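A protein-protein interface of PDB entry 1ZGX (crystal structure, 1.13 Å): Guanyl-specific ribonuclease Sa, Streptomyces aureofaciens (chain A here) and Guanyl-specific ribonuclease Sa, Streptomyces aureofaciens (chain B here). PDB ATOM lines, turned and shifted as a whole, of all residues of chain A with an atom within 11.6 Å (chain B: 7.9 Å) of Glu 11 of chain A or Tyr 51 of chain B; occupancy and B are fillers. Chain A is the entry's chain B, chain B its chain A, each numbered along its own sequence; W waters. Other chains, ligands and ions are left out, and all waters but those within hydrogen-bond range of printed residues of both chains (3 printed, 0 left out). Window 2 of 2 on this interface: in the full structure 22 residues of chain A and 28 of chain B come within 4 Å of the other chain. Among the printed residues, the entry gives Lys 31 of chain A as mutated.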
ATOM      1  N   ILE A   7      -1.068 -27.526  27.198  1.00  0.00           N
ATOM      2  CA  ILE A   7      -2.309 -26.980  26.572  1.00  0.00           C
ATOM      3  C   ILE A   7      -2.367 -27.434  25.084  1.00  0.00           C
ATOM      4  O   ILE A   7      -1.355 -27.345  24.344  1.00  0.00           O
ATOM      5  CB  ILE A   7      -2.417 -25.392  26.727  1.00  0.00           C
ATOM      6  CG1 ILE A   7      -2.677 -25.042  28.210  1.00  0.00           C
ATOM      7  CG2 ILE A   7      -3.511 -24.774  25.774  1.00  0.00           C
ATOM      8  CD1 ILE A   7      -2.645 -23.522  28.503  1.00  0.00           C
ATOM      9  N   ILE A   8      -3.569 -27.889  24.665  1.00  0.00           N
ATOM     10  CA  ILE A   8      -3.870 -28.131  23.237  1.00  0.00           C
ATOM     11  C   ILE A   8      -4.822 -26.990  22.742  1.00  0.00           C
ATOM     12  O   ILE A   8      -5.905 -26.750  23.360  1.00  0.00           O
ATOM     13  CB  ILE A   8      -4.547 -29.542  23.008  1.00  0.00           C
ATOM     14  CG1 ILE A   8      -3.658 -30.715  23.456  1.00  0.00           C
ATOM     15  CG2 ILE A   8      -5.065 -29.685  21.532  1.00  0.00           C
ATOM     16  CD1 ILE A   8      -2.321 -30.803  22.759  1.00  0.00           C
ATOM     17  N   THR A   9      -4.453 -26.346  21.604  1.00  0.00           N
ATOM     18  CA  THR A   9      -5.383 -25.409  20.908  1.00  0.00           C
ATOM     19  C   THR A   9      -6.201 -26.134  19.829  1.00  0.00           C
ATOM     20  O   THR A   9      -5.630 -26.984  19.093  1.00  0.00           O
ATOM     21  CB  THR A   9      -4.591 -24.232  20.267  1.00  0.00           C
ATOM     22  OG1 THR A   9      -3.697 -24.720  19.244  1.00  0.00           O
ATOM     23  CG2 THR A   9      -3.814 -23.370  21.287  1.00  0.00           C
ATOM     24  N   GLY A  10      -7.497 -25.777  19.709  1.00  0.00           N
ATOM     25  CA  GLY A  10      -8.271 -25.982  18.464  1.00  0.00           C
ATOM     26  C   GLY A  10      -8.476 -24.673  17.693  1.00  0.00           C
ATOM     27  O   GLY A  10      -8.048 -23.577  18.131  1.00  0.00           O
ATOM     28  N   GLU A  11      -9.204 -24.724  16.555  1.00  0.00           N
ATOM     29  CA  GLU A  11      -9.413 -23.524  15.683  1.00  0.00           C
ATOM     30  C   GLU A  11     -10.526 -22.519  16.130  1.00  0.00           C
ATOM     31  O   GLU A  11     -10.472 -21.299  15.731  1.00  0.00           O
ATOM     32  CB  GLU A  11      -9.674 -23.975  14.219  1.00  0.00           C
ATOM     33  CG  GLU A  11      -8.555 -24.727  13.566  1.00  0.00           C
ATOM     34  CD  GLU A  11      -8.935 -25.233  12.152  1.00  0.00           C
ATOM     35  OE1 GLU A  11     -10.128 -25.125  11.686  1.00  0.00           O
ATOM     36  OE2 GLU A  11      -8.029 -25.765  11.444  1.00  0.00           O
ATOM     37  N   ALA A  12     -11.525 -22.943  16.883  1.00  0.00           N
ATOM     38  CA  ALA A  12     -12.683 -22.118  17.227  1.00  0.00           C
ATOM     39  C   ALA A  12     -12.367 -21.099  18.358  1.00  0.00           C
ATOM     40  O   ALA A  12     -11.333 -21.211  19.082  1.00  0.00           O
ATOM     41  CB  ALA A  12     -13.846 -22.955  17.557  1.00  0.00           C
ATOM     42  N   THR A  13     -13.273 -20.097  18.519  1.00  0.00           N
ATOM     43  CA  THR A  13     -13.165 -18.971  19.408  1.00  0.00           C
ATOM     44  C   THR A  13     -13.053 -19.543  20.860  1.00  0.00           C
ATOM     45  O   THR A  13     -14.045 -20.087  21.392  1.00  0.00           O
ATOM     46  CB  THR A  13     -14.501 -18.007  19.187  1.00  0.00           C
ATOM     47  OG1 THR A  13     -14.728 -17.717  17.764  1.00  0.00           O
ATOM     48  CG2 THR A  13     -14.327 -16.718  19.827  1.00  0.00           C
ATOM     49  N   GLN A  14     -11.946 -19.272  21.603  1.00  0.00           N
ATOM     50  CA  GLN A  14     -11.633 -19.714  22.977  1.00  0.00           C
ATOM     51  C   GLN A  14     -11.512 -21.258  23.135  1.00  0.00           C
ATOM     52  O   GLN A  14     -11.625 -21.752  24.271  1.00  0.00           O
ATOM     53  CB  GLN A  14     -12.698 -19.164  24.031  1.00  0.00           C
ATOM     54  CG  GLN A  14     -13.090 -17.703  24.067  1.00  0.00           C
ATOM     55  CD  GLN A  14     -14.116 -17.380  25.203  1.00  0.00           C
ATOM     56  OE1 GLN A  14     -13.751 -17.090  26.374  1.00  0.00           O
ATOM     57  NE2 GLN A  14     -15.381 -17.392  24.887  1.00  0.00           N
ATOM     58  N   GLU A  15     -11.300 -22.006  22.036  1.00  0.00           N
ATOM     59  CA  GLU A  15     -11.247 -23.494  22.142  1.00  0.00           C
ATOM     60  C   GLU A  15      -9.813 -23.934  22.565  1.00  0.00           C
ATOM     61  O   GLU A  15      -8.905 -24.178  21.704  1.00  0.00           O
ATOM     62  CB  GLU A  15     -11.678 -24.143  20.796  1.00  0.00           C
ATOM     63  CG  GLU A  15     -11.750 -25.669  20.903  1.00  0.00           C
ATOM     64  CD  GLU A  15     -11.926 -26.423  19.532  1.00  0.00           C
ATOM     65  OE1 GLU A  15     -11.910 -25.763  18.456  1.00  0.00           O
ATOM     66  OE2 GLU A  15     -12.058 -27.681  19.603  1.00  0.00           O
ATOM     67  N   ASP A  16      -9.591 -24.030  23.885  1.00  0.00           N
ATOM     68  CA  ASP A  16      -8.300 -24.423  24.509  1.00  0.00           C
ATOM     69  C   ASP A  16      -8.590 -25.507  25.577  1.00  0.00           C
ATOM     70  O   ASP A  16      -9.544 -25.334  26.369  1.00  0.00           O
ATOM     71  CB  ASP A  16      -7.512 -23.150  24.957  1.00  0.00           C
ATOM     72  CG  ASP A  16      -7.127 -22.185  23.762  1.00  0.00           C
ATOM     73  OD1 ASP A  16      -6.822 -22.615  22.645  1.00  0.00           O
ATOM     74  OD2 ASP A  16      -7.008 -20.963  23.956  1.00  0.00           O
ATOM     75  N   TYR A  17      -7.748 -26.560  25.608  1.00  0.00           N
ATOM     76  CA  TYR A  17      -7.883 -27.715  26.530  1.00  0.00           C
ATOM     77  C   TYR A  17      -6.617 -27.828  27.414  1.00  0.00           C
ATOM     78  O   TYR A  17      -5.475 -27.679  26.899  1.00  0.00           O
ATOM     79  CB  TYR A  17      -8.085 -29.051  25.745  1.00  0.00           C
ATOM     80  CG  TYR A  17      -9.242 -29.065  24.722  1.00  0.00           C
ATOM     81  CD1 TYR A  17     -10.557 -29.451  25.073  1.00  0.00           C
ATOM     82  CD2 TYR A  17      -9.026 -28.634  23.395  1.00  0.00           C
ATOM     83  CE1 TYR A  17     -11.596 -29.447  24.142  1.00  0.00           C
ATOM     84  CE2 TYR A  17     -10.073 -28.617  22.450  1.00  0.00           C
ATOM     85  CZ  TYR A  17     -11.378 -29.036  22.833  1.00  0.00           C
ATOM     86  OH  TYR A  17     -12.454 -28.996  21.914  1.00  0.00           O
ATOM     87  N   LEU A  28     -11.942 -28.612  29.142  1.00  0.00           N
ATOM     88  CA  LEU A  28     -12.026 -27.284  28.469  1.00  0.00           C
ATOM     89  C   LEU A  28     -11.652 -26.188  29.479  1.00  0.00           C
ATOM     90  O   LEU A  28     -12.110 -26.217  30.647  1.00  0.00           O
ATOM     91  CB  LEU A  28     -13.414 -27.074  27.869  1.00  0.00           C
ATOM     92  CG  LEU A  28     -13.709 -27.445  26.382  1.00  0.00           C
ATOM     93  CD1 LEU A  28     -15.179 -27.522  26.051  1.00  0.00           C
ATOM     94  CD2 LEU A  28     -12.998 -26.452  25.455  1.00  0.00           C
ATOM     95  N   LYS A  31     -11.921 -19.360  30.605  1.00  0.00           N
ATOM     96  CA  LYS A  31     -11.144 -18.133  30.824  1.00  0.00           C
ATOM     97  C   LYS A  31     -11.918 -17.018  31.542  1.00  0.00           C
ATOM     98  O   LYS A  31     -11.332 -15.951  31.803  1.00  0.00           O
ATOM     99  CB  LYS A  31     -10.481 -17.611  29.488  1.00  0.00           C
ATOM    100  CG  LYS A  31      -9.666 -18.641  28.751  1.00  0.00           C
ATOM    101  CD  LYS A  31      -9.245 -18.179  27.296  1.00  0.00           C
ATOM    102  CE  LYS A  31      -8.607 -19.231  26.514  1.00  0.00           C
ATOM    103  NZ  LYS A  31      -8.122 -18.618  25.267  1.00  0.00           N
ATOM    104  N   VAL B  36       2.110 -30.056  15.485  1.00  0.00           N
ATOM    105  CA  VAL B  36       0.762 -30.647  15.349  1.00  0.00           C
ATOM    106  C   VAL B  36       0.551 -31.772  16.424  1.00  0.00           C
ATOM    107  O   VAL B  36       1.449 -32.640  16.633  1.00  0.00           O
ATOM    108  CB  VAL B  36       0.526 -31.150  13.889  1.00  0.00           C
ATOM    109  CG1 VAL B  36      -0.814 -31.905  13.789  1.00  0.00           C
ATOM    110  CG2 VAL B  36       0.569 -29.976  12.862  1.00  0.00           C
ATOM    111  N   PHE B  37      -0.628 -31.742  17.087  1.00  0.00           N
ATOM    112  CA  PHE B  37      -1.081 -32.844  17.991  1.00  0.00           C
ATOM    113  C   PHE B  37      -1.977 -33.810  17.151  1.00  0.00           C
ATOM    114  O   PHE B  37      -2.982 -33.382  16.531  1.00  0.00           O
ATOM    115  CB  PHE B  37      -1.875 -32.272  19.199  1.00  0.00           C
ATOM    116  CG  PHE B  37      -2.449 -33.357  20.158  1.00  0.00           C
ATOM    117  CD1 PHE B  37      -1.575 -34.170  20.911  1.00  0.00           C
ATOM    118  CD2 PHE B  37      -3.827 -33.572  20.279  1.00  0.00           C
ATOM    119  CE1 PHE B  37      -2.061 -35.193  21.742  1.00  0.00           C
ATOM    120  CE2 PHE B  37      -4.332 -34.554  21.166  1.00  0.00           C
ATOM    121  CZ  PHE B  37      -3.421 -35.376  21.884  1.00  0.00           C
ATOM    122  N   LEU B  44     -10.179 -36.208  22.201  1.00  0.00           N
ATOM    123  CA  LEU B  44     -10.804 -34.991  21.670  1.00  0.00           C
ATOM    124  C   LEU B  44     -11.693 -35.335  20.441  1.00  0.00           C
ATOM    125  O   LEU B  44     -11.446 -36.373  19.787  1.00  0.00           O
ATOM    126  CB  LEU B  44      -9.760 -33.894  21.310  1.00  0.00           C
ATOM    127  CG  LEU B  44      -8.772 -33.480  22.473  1.00  0.00           C
ATOM    128  CD1 LEU B  44      -7.732 -32.466  21.964  1.00  0.00           C
ATOM    129  CD2 LEU B  44      -9.539 -32.833  23.671  1.00  0.00           C
ATOM    130  N   PRO B  45     -12.669 -34.483  20.093  1.00  0.00           N
ATOM    131  CA  PRO B  45     -13.480 -34.735  18.864  1.00  0.00           C
ATOM    132  C   PRO B  45     -12.600 -34.910  17.597  1.00  0.00           C
ATOM    133  O   PRO B  45     -11.573 -34.160  17.409  1.00  0.00           O
ATOM    134  CB  PRO B  45     -14.414 -33.479  18.806  1.00  0.00           C
ATOM    135  CG  PRO B  45     -14.564 -33.081  20.232  1.00  0.00           C
ATOM    136  CD  PRO B  45     -13.180 -33.293  20.823  1.00  0.00           C
ATOM    137  N   THR B  46     -12.942 -35.851  16.699  1.00  0.00           N
ATOM    138  CA  THR B  46     -12.165 -36.042  15.459  1.00  0.00           C
ATOM    139  C   THR B  46     -12.228 -34.786  14.558  1.00  0.00           C
ATOM    140  O   THR B  46     -13.341 -34.233  14.320  1.00  0.00           O
ATOM    141  CB  THR B  46     -12.712 -37.297  14.650  1.00  0.00           C
ATOM    142  OG1 THR B  46     -12.744 -38.466  15.505  1.00  0.00           O
ATOM    143  CG2 THR B  46     -11.824 -37.653  13.446  1.00  0.00           C
ATOM    144  N   GLN B  47     -11.040 -34.338  14.081  1.00  0.00           N
ATOM    145  CA  GLN B  47     -10.913 -33.157  13.177  1.00  0.00           C
ATOM    146  C   GLN B  47      -9.762 -33.409  12.156  1.00  0.00           C
ATOM    147  O   GLN B  47      -9.007 -34.410  12.275  1.00  0.00           O
ATOM    148  CB  GLN B  47     -10.642 -31.842  13.991  1.00  0.00           C
ATOM    149  CG  GLN B  47     -11.675 -31.434  14.994  1.00  0.00           C
ATOM    150  CD  GLN B  47     -12.987 -30.826  14.404  1.00  0.00           C
ATOM    151  OE1 GLN B  47     -13.223 -30.850  13.161  1.00  0.00           O
ATOM    152  NE2 GLN B  47     -13.850 -30.271  15.281  1.00  0.00           N
ATOM    153  N   SER B  48      -9.587 -32.544  11.153  1.00  0.00           N
ATOM    154  CA  SER B  48      -8.525 -32.703  10.166  1.00  0.00           C
ATOM    155  C   SER B  48      -7.120 -32.771  10.841  1.00  0.00           C
ATOM    156  O   SER B  48      -6.896 -32.170  11.944  1.00  0.00           O
ATOM    157  CB  SER B  48      -8.521 -31.496   9.231  1.00  0.00           C
ATOM    158  OG  SER B  48      -7.699 -31.770   8.180  1.00  0.00           O
ATOM    159  N   TYR B  49      -6.126 -33.354  10.145  1.00  0.00           N
ATOM    160  CA  TYR B  49      -4.713 -33.310  10.583  1.00  0.00           C
ATOM    161  C   TYR B  49      -4.250 -31.840  10.505  1.00  0.00           C
ATOM    162  O   TYR B  49      -4.310 -31.246   9.424  1.00  0.00           O
ATOM    163  CB  TYR B  49      -3.833 -34.234   9.661  1.00  0.00           C
ATOM    164  CG  TYR B  49      -2.369 -34.208  10.059  1.00  0.00           C
ATOM    165  CD1 TYR B  49      -1.884 -34.949  11.164  1.00  0.00           C
ATOM    166  CD2 TYR B  49      -1.464 -33.413   9.400  1.00  0.00           C
ATOM    167  CE1 TYR B  49      -0.527 -34.901  11.580  1.00  0.00           C
ATOM    168  CE2 TYR B  49      -0.058 -33.380   9.818  1.00  0.00           C
ATOM    169  CZ  TYR B  49       0.351 -34.116  10.905  1.00  0.00           C
ATOM    170  OH  TYR B  49       1.709 -34.095  11.302  1.00  0.00           O
ATOM    171  N   GLY B  50      -3.770 -31.256  11.605  1.00  0.00           N
ATOM    172  CA  GLY B  50      -3.385 -29.835  11.674  1.00  0.00           C
ATOM    173  C   GLY B  50      -4.401 -28.923  12.383  1.00  0.00           C
ATOM    174  O   GLY B  50      -4.089 -27.738  12.649  1.00  0.00           O
ATOM    175  N   TYR B  51      -5.614 -29.423  12.725  1.00  0.00           N
ATOM    176  CA  TYR B  51      -6.607 -28.661  13.501  1.00  0.00           C
ATOM    177  C   TYR B  51      -6.076 -28.343  14.955  1.00  0.00           C
ATOM    178  O   TYR B  51      -6.393 -27.266  15.513  1.00  0.00           O
ATOM    179  CB  TYR B  51      -7.956 -29.446  13.559  1.00  0.00           C
ATOM    180  CG  TYR B  51      -9.129 -28.724  14.256  1.00  0.00           C
ATOM    181  CD1 TYR B  51      -9.278 -28.711  15.645  1.00  0.00           C
ATOM    182  CD2 TYR B  51     -10.137 -28.064  13.499  1.00  0.00           C
ATOM    183  CE1 TYR B  51     -10.370 -28.082  16.286  1.00  0.00           C
ATOM    184  CE2 TYR B  51     -11.203 -27.412  14.100  1.00  0.00           C
ATOM    185  CZ  TYR B  51     -11.338 -27.403  15.518  1.00  0.00           C
ATOM    186  OH  TYR B  51     -12.395 -26.698  16.079  1.00  0.00           O
ATOM    187  N   TYR B  52      -5.375 -29.316  15.545  1.00  0.00           N
ATOM    188  CA  TYR B  52      -4.877 -29.247  16.954  1.00  0.00           C
ATOM    189  C   TYR B  52      -3.328 -29.032  16.980  1.00  0.00           C
ATOM    190  O   TYR B  52      -2.583 -29.680  16.199  1.00  0.00           O
ATOM    191  CB  TYR B  52      -5.222 -30.537  17.724  1.00  0.00           C
ATOM    192  CG  TYR B  52      -6.725 -30.872  17.905  1.00  0.00           C
ATOM    193  CD1 TYR B  52      -7.561 -30.070  18.705  1.00  0.00           C
ATOM    194  CD2 TYR B  52      -7.298 -32.015  17.293  1.00  0.00           C
ATOM    195  CE1 TYR B  52      -8.942 -30.375  18.899  1.00  0.00           C
ATOM    196  CE2 TYR B  52      -8.658 -32.328  17.494  1.00  0.00           C
ATOM    197  CZ  TYR B  52      -9.483 -31.531  18.295  1.00  0.00           C
ATOM    198  OH  TYR B  52     -10.841 -31.816  18.552  1.00  0.00           O
ATOM    199  N   HIS B  53      -2.856 -28.169  17.920  1.00  0.00           N
ATOM    200  CA  HIS B  53      -1.409 -27.955  18.191  1.00  0.00           C
ATOM    201  C   HIS B  53      -1.135 -28.045  19.727  1.00  0.00           C
ATOM    202  O   HIS B  53      -2.019 -27.743  20.534  1.00  0.00           O
ATOM    203  CB  HIS B  53      -0.874 -26.583  17.629  1.00  0.00           C
ATOM    204  CG  HIS B  53      -0.976 -26.446  16.125  1.00  0.00           C
ATOM    205  ND1 HIS B  53       0.010 -26.637  15.167  1.00  0.00           N
ATOM    206  CD2 HIS B  53      -2.112 -26.112  15.433  1.00  0.00           C
ATOM    207  CE1 HIS B  53      -0.528 -26.433  13.939  1.00  0.00           C
ATOM    208  NE2 HIS B  53      -1.809 -26.138  14.081  1.00  0.00           N
HETATM  209  O   HOH W   1      -4.626 -25.368  16.578  1.00  0.00           O
HETATM  210  O   HOH W   2     -13.034 -29.916  18.203  1.00  0.00           O
HETATM  211  O   HOH W   3      -5.205 -25.259  12.201  1.00  0.00           O
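OH of Tyr 51 of chain B is in hydrogen-bond range of OE1 of Glu 15 of chain A (2.6 Å).
The backbone carbonyl oxygen (O) of His 53 of chain B lies within hydrogen-bond range of the backbone NH (N) of Thr 9 of chain A, 3.0 Å away.
The backbone carbonyl oxygen (O) of Gly 50 of chain B lies within hydrogen-bond range of a ring nitrogen (NE2) of His 53 of chain B (3.1 Å).
N of Tyr 17 of chain A sits at hydrogen-bond distance from O of Ile 8 of chain A.
The backbone carbonyl oxygen (O) of Glu 15 of chain A is in hydrogen-bond range of the backbone NH (N) of Gly 10 of chain A, at 2.9 Å.
The side-chain carboxylate (OE1) of Glu 15 of chain A sits at hydrogen-bond distance from the backbone NH (N) of Glu 11 of chain A (3.5 Å).
OE1 of Glu 15 of chain A lies within hydrogen-bond range of N of Ala 12 of chain A (3.3 Å).
OH of Tyr 17 of chain A lies within hydrogen-bond range of OE2 of Glu 15 of chain A, at 2.7 Å.
Among the printed residues, pairs that only touch across the chains: Thr 9 of chain A with Tyr 52 of chain B (3.2 Å), Ile 8 of chain A with His 53 of chain B (3.3 Å), Glu 11 of chain A with Tyr 51 of chain B (3.4 Å), Ile 8 of chain A with Phe 37 of chain B (3.6 Å), Thr 9 of chain A with Tyr 51 of chain B (3.7 Å), Gly 10 of chain A with Tyr 51 of chain B (3.7 Å), Ile 8 of chain A with Tyr 52 of chain B (3.8 Å), Tyr 17 of chain A with Leu 44 of chain B (3.8 Å), Ile 8 of chain A with Leu 44 of chain B (3.9 Å), Ile 7 of chain A with His 53 of chain B (3.9 Å) and Ala 12 of chain A with Tyr 51 of chain B (3.9 Å).
Glu 11 of chain A touches just one residue of chain B: Tyr 51 (3.4 Å).
Of chain A, only Thr 9 (3.7 Å), Gly 10 (3.7 Å), Glu 11 (3.4 Å), Ala 12 (3.9 Å) and Glu 15 (2.6 Å) come within 4 Å of Tyr 51 of chain B.
Ala 12 of chain A touches just one residue of chain B: Tyr 51 (3.9 Å).
No residue of chain A comes within 4 Å of Gly 50 of chain B.
Tyr 52 of chain B touches just these residues of chain A: Ile 8 and Thr 9.
His 53 of chain B touches three residues of chain A.
Of the printed residues of chain A, Leu 44 of chain B touches Ile 8 (3.9 Å) and Tyr 17 (3.8 Å).
Printed residues of chain B within 4 Å of Glu 15 of chain A: Tyr 51.
Of the printed residues of chain A, Phe 37 of chain B touches Ile 8.
Of the printed residues of chain B, Tyr 17 of chain A touches Leu 44 (3.8 Å).
The nearest printed residue of chain A that does not touch Leu 44 of chain B is Thr 9 of chain A (6.5 Å).
Of the 13 printed residues of chain A, 8 touch a printed residue of chain B.
Along chain A the printed residues that touch a printed residue of chain B span positions 7 to 17.
Of the 12 printed residues of chain B, 5 touch a printed residue of chain A.
Printed residues of chain B that touch a printed residue of chain A: Phe 37, Leu 44, Tyr 51, Tyr 52 and His 53.
Among the printed residues, 13 pairs touch across the chains.
Among the printed residues, no Asp or Glu carboxylate lies within 4 Å of a Lys or Arg side-chain nitrogen of the other chain.
Water W3 lies within hydrogen-bond range of the backbone carbonyl oxygen (O) of Gly 50 of chain B (2.8 Å) and the side-chain carboxylate (OE2) of Glu 11 of chain A (3.0 Å).
Water W1 bridges O of Tyr 51 of chain B (2.8 Å) and OG1 of Thr 9 of chain A (2.9 Å).
Water W2 lies within hydrogen-bond range of the side-chain carboxylate of Glu 15 of chain A (2.8 Å), the side-chain hydroxyl of Tyr 52 of chain B (2.9 Å) and the side-chain amide nitrogen of Gln 47 of chain B (3.1 Å).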
